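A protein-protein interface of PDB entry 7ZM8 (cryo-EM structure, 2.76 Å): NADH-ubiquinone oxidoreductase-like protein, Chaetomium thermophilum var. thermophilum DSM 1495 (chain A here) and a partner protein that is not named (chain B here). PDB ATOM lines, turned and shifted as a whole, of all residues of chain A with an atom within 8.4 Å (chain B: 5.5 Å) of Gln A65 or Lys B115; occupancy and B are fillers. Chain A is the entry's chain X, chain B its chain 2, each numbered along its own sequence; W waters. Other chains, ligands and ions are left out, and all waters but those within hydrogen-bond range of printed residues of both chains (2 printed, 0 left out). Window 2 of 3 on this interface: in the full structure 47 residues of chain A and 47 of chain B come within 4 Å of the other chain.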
ATOM      1  N   GLU A  59       6.553  20.011 -11.309  1.00  0.00           N
ATOM      2  CA  GLU A  59       5.277  19.440 -10.781  1.00  0.00           C
ATOM      3  C   GLU A  59       5.006  18.098 -11.451  1.00  0.00           C
ATOM      4  O   GLU A  59       4.582  17.171 -10.776  1.00  0.00           O
ATOM      5  CB  GLU A  59       4.107  20.397 -10.962  1.00  0.00           C
ATOM      6  CG  GLU A  59       2.832  19.940 -10.278  1.00  0.00           C
ATOM      7  CD  GLU A  59       2.810  20.028  -8.761  1.00  0.00           C
ATOM      8  OE1 GLU A  59       3.826  20.431  -8.173  1.00  0.00           O
ATOM      9  OE2 GLU A  59       1.768  19.705  -8.171  1.00  0.00           O
ATOM     10  N   ARG A  60       5.133  18.062 -12.771  1.00  0.00           N
ATOM     11  CA  ARG A  60       4.904  16.825 -13.547  1.00  0.00           C
ATOM     12  C   ARG A  60       5.876  15.733 -13.089  1.00  0.00           C
ATOM     13  O   ARG A  60       5.429  14.597 -12.917  1.00  0.00           O
ATOM     14  CB  ARG A  60       4.987  17.191 -15.033  1.00  0.00           C
ATOM     15  CG  ARG A  60       4.638  16.065 -15.992  1.00  0.00           C
ATOM     16  CD  ARG A  60       3.199  15.636 -15.805  1.00  0.00           C
ATOM     17  NE  ARG A  60       2.238  16.676 -16.135  1.00  0.00           N
ATOM     18  CZ  ARG A  60       1.630  16.787 -17.307  1.00  0.00           C
ATOM     19  NH1 ARG A  60       1.877  15.914 -18.268  1.00  0.00           N
ATOM     20  NH2 ARG A  60       0.767  17.766 -17.513  1.00  0.00           N
ATOM     21  N   ILE A  61       7.162  16.058 -12.959  1.00  0.00           N
ATOM     22  CA  ILE A  61       8.181  15.004 -12.677  1.00  0.00           C
ATOM     23  C   ILE A  61       8.153  14.597 -11.202  1.00  0.00           C
ATOM     24  O   ILE A  61       7.929  13.405 -10.938  1.00  0.00           O
ATOM     25  CB  ILE A  61       9.584  15.394 -13.189  1.00  0.00           C
ATOM     26  CG1 ILE A  61       9.694  15.282 -14.712  1.00  0.00           C
ATOM     27  CG2 ILE A  61      10.636  14.522 -12.534  1.00  0.00           C
ATOM     28  CD1 ILE A  61       8.965  16.337 -15.493  1.00  0.00           C
ATOM     29  N   SER A  62       8.411  15.521 -10.279  1.00  0.00           N
ATOM     30  CA  SER A  62       8.263  15.181  -8.840  1.00  0.00           C
ATOM     31  C   SER A  62       7.006  15.871  -8.315  1.00  0.00           C
ATOM     32  O   SER A  62       7.078  17.059  -7.970  1.00  0.00           O
ATOM     33  CB  SER A  62       9.477  15.592  -8.068  1.00  0.00           C
ATOM     34  OG  SER A  62       9.861  16.912  -8.417  1.00  0.00           O
ATOM     35  N   PRO A  63       5.857  15.181  -8.204  1.00  0.00           N
ATOM     36  CA  PRO A  63       4.615  15.841  -7.800  1.00  0.00           C
ATOM     37  C   PRO A  63       4.591  16.314  -6.339  1.00  0.00           C
ATOM     38  O   PRO A  63       4.988  15.568  -5.479  1.00  0.00           O
ATOM     39  CB  PRO A  63       3.550  14.787  -8.137  1.00  0.00           C
ATOM     40  CG  PRO A  63       4.245  13.812  -9.060  1.00  0.00           C
ATOM     41  CD  PRO A  63       5.665  13.775  -8.545  1.00  0.00           C
ATOM     42  N   SER A  64       4.119  17.534  -6.103  1.00  0.00           N
ATOM     43  CA  SER A  64       4.062  18.120  -4.742  1.00  0.00           C
ATOM     44  C   SER A  64       3.066  17.452  -3.810  1.00  0.00           C
ATOM     45  O   SER A  64       3.275  17.588  -2.599  1.00  0.00           O
ATOM     46  CB  SER A  64       3.785  19.589  -4.846  1.00  0.00           C
ATOM     47  OG  SER A  64       2.519  19.836  -5.434  1.00  0.00           O
ATOM     48  N   GLN A  65       2.000  16.843  -4.322  1.00  0.00           N
ATOM     49  CA  GLN A  65       1.014  16.134  -3.469  1.00  0.00           C
ATOM     50  C   GLN A  65       0.265  17.162  -2.635  1.00  0.00           C
ATOM     51  O   GLN A  65      -0.120  16.827  -1.510  1.00  0.00           O
ATOM     52  CB  GLN A  65       1.682  15.070  -2.594  1.00  0.00           C
ATOM     53  CG  GLN A  65       2.548  14.081  -3.362  1.00  0.00           C
ATOM     54  CD  GLN A  65       1.768  13.310  -4.396  1.00  0.00           C
ATOM     55  OE1 GLN A  65       0.751  12.690  -4.105  1.00  0.00           O
ATOM     56  NE2 GLN A  65       2.260  13.328  -5.622  1.00  0.00           N
ATOM     57  N   VAL A  66       0.087  18.367  -3.171  1.00  0.00           N
ATOM     58  CA  VAL A  66      -0.602  19.470  -2.447  1.00  0.00           C
ATOM     59  C   VAL A  66      -2.098  19.255  -2.627  1.00  0.00           C
ATOM     60  O   VAL A  66      -2.463  18.323  -3.369  1.00  0.00           O
ATOM     61  CB  VAL A  66      -0.168  20.851  -2.970  1.00  0.00           C
ATOM     62  CG1 VAL A  66      -0.660  21.134  -4.378  1.00  0.00           C
ATOM     63  CG2 VAL A  66      -0.500  21.996  -2.029  1.00  0.00           C
ATOM     64  N   GLY A  67      -2.921  20.089  -1.997  1.00  0.00           N
ATOM     65  CA  GLY A  67      -4.378  20.013  -2.127  1.00  0.00           C
ATOM     66  C   GLY A  67      -4.886  20.692  -3.367  1.00  0.00           C
ATOM     67  O   GLY A  67      -4.059  21.066  -4.194  1.00  0.00           O
ATOM     68  N   ARG A  68      -6.194  20.904  -3.468  1.00  0.00           N
ATOM     69  CA  ARG A  68      -6.830  21.381  -4.711  1.00  0.00           C
ATOM     70  C   ARG A  68      -6.389  22.749  -5.232  1.00  0.00           C
ATOM     71  O   ARG A  68      -6.230  22.847  -6.460  1.00  0.00           O
ATOM     72  CB  ARG A  68      -8.342  21.311  -4.529  1.00  0.00           C
ATOM     73  CG  ARG A  68      -8.867  19.906  -4.277  1.00  0.00           C
ATOM     74  CD  ARG A  68     -10.358  19.887  -4.001  1.00  0.00           C
ATOM     75  NE  ARG A  68     -10.880  18.533  -3.876  1.00  0.00           N
ATOM     76  CZ  ARG A  68     -10.969  17.859  -2.734  1.00  0.00           C
ATOM     77  NH1 ARG A  68     -10.569  18.413  -1.602  1.00  0.00           N
ATOM     78  NH2 ARG A  68     -11.458  16.632  -2.728  1.00  0.00           N
ATOM     79  N   PHE A  71      -1.448  24.587  -6.302  1.00  0.00           N
ATOM     80  CA  PHE A  71      -0.578  24.777  -7.474  1.00  0.00           C
ATOM     81  C   PHE A  71      -0.943  26.080  -8.170  1.00  0.00           C
ATOM     82  O   PHE A  71      -0.032  26.778  -8.604  1.00  0.00           O
ATOM     83  CB  PHE A  71      -0.505  23.519  -8.336  1.00  0.00           C
ATOM     84  CG  PHE A  71       0.632  23.562  -9.321  1.00  0.00           C
ATOM     85  CD1 PHE A  71       1.943  23.608  -8.878  1.00  0.00           C
ATOM     86  CD2 PHE A  71       0.395  23.606 -10.683  1.00  0.00           C
ATOM     87  CE1 PHE A  71       2.993  23.676  -9.776  1.00  0.00           C
ATOM     88  CE2 PHE A  71       1.448  23.668 -11.579  1.00  0.00           C
ATOM     89  CZ  PHE A  71       2.744  23.705 -11.125  1.00  0.00           C
ATOM     90  N   ASP B  20       0.495  22.492   3.570  1.00  0.00           N
ATOM     91  CA  ASP B  20       0.785  21.630   2.394  1.00  0.00           C
ATOM     92  C   ASP B  20       1.415  22.503   1.311  1.00  0.00           C
ATOM     93  O   ASP B  20       2.009  21.947   0.381  1.00  0.00           O
ATOM     94  CB  ASP B  20      -0.467  20.880   1.929  1.00  0.00           C
ATOM     95  CG  ASP B  20      -1.626  21.738   1.453  1.00  0.00           C
ATOM     96  OD1 ASP B  20      -1.567  22.967   1.613  1.00  0.00           O
ATOM     97  OD2 ASP B  20      -2.584  21.161   0.917  1.00  0.00           O
ATOM     98  N   TYR B  85      10.469  15.511  -1.675  1.00  0.00           N
ATOM     99  CA  TYR B  85      10.253  14.477  -0.641  1.00  0.00           C
ATOM    100  C   TYR B  85      11.497  13.608  -0.529  1.00  0.00           C
ATOM    101  O   TYR B  85      12.123  13.304  -1.541  1.00  0.00           O
ATOM    102  CB  TYR B  85       8.968  13.708  -0.935  1.00  0.00           C
ATOM    103  CG  TYR B  85       7.720  14.523  -0.732  1.00  0.00           C
ATOM    104  CD1 TYR B  85       7.316  14.897   0.537  1.00  0.00           C
ATOM    105  CD2 TYR B  85       6.949  14.925  -1.805  1.00  0.00           C
ATOM    106  CE1 TYR B  85       6.177  15.655   0.732  1.00  0.00           C
ATOM    107  CE2 TYR B  85       5.806  15.682  -1.628  1.00  0.00           C
ATOM    108  CZ  TYR B  85       5.416  16.044  -0.355  1.00  0.00           C
ATOM    109  OH  TYR B  85       4.291  16.786  -0.164  1.00  0.00           O
ATOM    110  N   ARG B 109       1.084   7.611  -1.229  1.00  0.00           N
ATOM    111  CA  ARG B 109       2.473   8.110  -1.069  1.00  0.00           C
ATOM    112  C   ARG B 109       2.738   8.660   0.333  1.00  0.00           C
ATOM    113  O   ARG B 109       3.917   8.791   0.635  1.00  0.00           O
ATOM    114  CB  ARG B 109       2.750   9.235  -2.078  1.00  0.00           C
ATOM    115  CG  ARG B 109       2.164   9.047  -3.466  1.00  0.00           C
ATOM    116  CD  ARG B 109       2.993   9.853  -4.444  1.00  0.00           C
ATOM    117  NE  ARG B 109       2.414   9.861  -5.777  1.00  0.00           N
ATOM    118  CZ  ARG B 109       3.057  10.252  -6.870  1.00  0.00           C
ATOM    119  NH1 ARG B 109       4.314  10.651  -6.793  1.00  0.00           N
ATOM    120  NH2 ARG B 109       2.445  10.233  -8.038  1.00  0.00           N
ATOM    121  N   THR B 110       1.730   8.820   1.195  1.00  0.00           N
ATOM    122  CA  THR B 110       1.911   9.540   2.485  1.00  0.00           C
ATOM    123  C   THR B 110       2.969   8.944   3.420  1.00  0.00           C
ATOM    124  O   THR B 110       3.845   9.695   3.843  1.00  0.00           O
ATOM    125  CB  THR B 110       0.558   9.706   3.192  1.00  0.00           C
ATOM    126  OG1 THR B 110      -0.324  10.284   2.233  1.00  0.00           O
ATOM    127  CG2 THR B 110       0.618  10.571   4.429  1.00  0.00           C
ATOM    128  N   ILE B 113       6.705   8.622   1.499  1.00  0.00           N
ATOM    129  CA  ILE B 113       7.496   9.817   1.223  1.00  0.00           C
ATOM    130  C   ILE B 113       7.617  10.735   2.427  1.00  0.00           C
ATOM    131  O   ILE B 113       8.314  11.753   2.340  1.00  0.00           O
ATOM    132  CB  ILE B 113       6.930  10.609   0.022  1.00  0.00           C
ATOM    133  CG1 ILE B 113       5.622  11.307   0.399  1.00  0.00           C
ATOM    134  CG2 ILE B 113       6.762   9.711  -1.196  1.00  0.00           C
ATOM    135  CD1 ILE B 113       4.914  11.934  -0.753  1.00  0.00           C
ATOM    136  N   ASN B 114       6.925  10.452   3.536  1.00  0.00           N
ATOM    137  CA  ASN B 114       6.881  11.343   4.735  1.00  0.00           C
ATOM    138  C   ASN B 114       6.339  12.703   4.296  1.00  0.00           C
ATOM    139  O   ASN B 114       7.037  13.704   4.507  1.00  0.00           O
ATOM    140  CB  ASN B 114       8.230  11.451   5.454  1.00  0.00           C
ATOM    141  CG  ASN B 114       8.130  11.889   6.898  1.00  0.00           C
ATOM    142  OD1 ASN B 114       7.049  11.911   7.478  1.00  0.00           O
ATOM    143  ND2 ASN B 114       9.261  12.226   7.493  1.00  0.00           N
ATOM    144  N   LYS B 115       5.118  12.736   3.757  1.00  0.00           N
ATOM    145  CA  LYS B 115       4.522  13.976   3.212  1.00  0.00           C
ATOM    146  C   LYS B 115       4.350  15.001   4.318  1.00  0.00           C
ATOM    147  O   LYS B 115       4.603  16.178   4.072  1.00  0.00           O
ATOM    148  CB  LYS B 115       3.152  13.610   2.643  1.00  0.00           C
ATOM    149  CG  LYS B 115       2.495  14.679   1.783  1.00  0.00           C
ATOM    150  CD  LYS B 115       1.284  14.185   1.027  1.00  0.00           C
ATOM    151  CE  LYS B 115       0.137  13.794   1.930  1.00  0.00           C
ATOM    152  NZ  LYS B 115      -1.058  13.395   1.154  1.00  0.00           N
ATOM    153  N   MET B 116       3.940  14.550   5.501  1.00  0.00           N
ATOM    154  CA  MET B 116       3.633  15.481   6.604  1.00  0.00           C
ATOM    155  C   MET B 116       4.738  15.449   7.661  1.00  0.00           C
ATOM    156  O   MET B 116       4.407  15.543   8.853  1.00  0.00           O
ATOM    157  CB  MET B 116       2.275  15.120   7.202  1.00  0.00           C
ATOM    158  CG  MET B 116       1.195  14.975   6.158  1.00  0.00           C
ATOM    159  SD  MET B 116      -0.430  14.732   6.897  1.00  0.00           S
ATOM    160  CE  MET B 116      -1.363  14.180   5.471  1.00  0.00           C
ATOM    161  N   GLY B 117       5.997  15.355   7.240  1.00  0.00           N
ATOM    162  CA  GLY B 117       7.137  15.451   8.171  1.00  0.00           C
ATOM    163  C   GLY B 117       7.323  16.880   8.642  1.00  0.00           C
ATOM    164  O   GLY B 117       6.832  17.782   7.957  1.00  0.00           O
ATOM    165  N   MET B 120       8.522  19.506   6.179  1.00  0.00           N
ATOM    166  CA  MET B 120       7.589  19.800   5.073  1.00  0.00           C
ATOM    167  C   MET B 120       6.348  20.553   5.565  1.00  0.00           C
ATOM    168  O   MET B 120       5.338  20.492   4.858  1.00  0.00           O
ATOM    169  CB  MET B 120       7.154  18.479   4.435  1.00  0.00           C
ATOM    170  CG  MET B 120       8.295  17.666   3.870  1.00  0.00           C
ATOM    171  SD  MET B 120       9.241  18.560   2.612  1.00  0.00           S
ATOM    172  CE  MET B 120      10.244  17.230   1.962  1.00  0.00           C
ATOM    173  N   LYS B 121       6.432  21.261   6.690  1.00  0.00           N
ATOM    174  CA  LYS B 121       5.211  21.891   7.264  1.00  0.00           C
ATOM    175  C   LYS B 121       5.521  23.272   7.835  1.00  0.00           C
ATOM    176  O   LYS B 121       4.644  23.816   8.519  1.00  0.00           O
ATOM    177  CB  LYS B 121       4.567  20.971   8.308  1.00  0.00           C
ATOM    178  CG  LYS B 121       3.731  19.832   7.742  1.00  0.00           C
ATOM    179  CD  LYS B 121       3.274  18.841   8.782  1.00  0.00           C
ATOM    180  CE  LYS B 121       2.493  19.480   9.909  1.00  0.00           C
ATOM    181  NZ  LYS B 121       1.807  18.468  10.746  1.00  0.00           N
HETATM  182  O   HOH W   1       5.849  12.938  -4.860  1.00  0.00           O
HETATM  183  O   HOH W   2       0.036  11.312  -1.323  1.00  0.00           O
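The backbone carbonyl oxygen (O) of Ser A64 lies within hydrogen-bond range of the side-chain hydroxyl (OH) of Tyr B85, 2.8 Å away.
NE2 of Gln A65 sits close to NE of Arg B109.
The side-chain carboxylate (OD2) of Asp B20 is in hydrogen-bond range of the backbone NH (N) of Gly A67, 3.1 Å away.
The side-chain carboxylate of Glu A59 sits at hydrogen-bond distance from the side-chain hydroxyl of Ser A64 (2.8 Å).
The backbone NH of Lys B115 sits at hydrogen-bond distance from the backbone carbonyl oxygen of Thr B110.
Among the printed residues, merely in contact across the chains: Pro A63 with Tyr B85 (3.9 Å), Pro A63 with Arg B109 (3.8 Å), Gln A65 with Tyr B85 (3.96 Å), Gln A65 with Lys B115 (3.7 Å) and Val A66 with Asp B20 (3.5 Å).
Of chain B, only Tyr B85 (3.96 Å), Arg B109 (3.4 Å) and Lys B115 (3.7 Å) come within 4 Å of Gln A65.
Lys B115 touches just one residue of chain A: Gln A65 (3.7 Å).
Printed residues of chain B within 4 Å of Val A66: Asp B20 (3.5 Å).
Of the printed residues of chain A, Arg B109 touches Pro A63 and Gln A65.
Of the printed residues of chain B, Ser A64 touches Tyr B85.
Printed residues of chain A within 4 Å of Asp B20: Val A66 and Gly A67.
Of the printed residues of chain B, Gly A67 touches Asp B20.
Ile A61 touches none of the printed residues of chain B.
The nearest residue of chain A that does not touch Lys B115 is Ser A64 (5.3 Å).
The nearest printed residue of chain B that does not touch Gly A67 is Lys B115 (7.6 Å).
Hydrophobic or aromatic side chains of chain B within 4 Å of the printed part of chain A: Tyr B85.
Hydrophobic or aromatic side chains of chain A that line the printed part of chain B: Pro A63 and Val A66.
Among the printed residues, 8 pairs touch across the chains.
Among the printed residues, no Asp or Glu carboxylate lies within 4 Å of a Lys or Arg side-chain nitrogen of the other chain.
Water W1 lies within hydrogen-bond range of O of Pro A63 (2.8 Å) and NH1 of Arg B109 (3.4 Å).
Water W2 bridges the side-chain amide oxygen of Gln A65 (3.2 Å) and the side-chain amino group of Lys B115 (3.4 Å).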
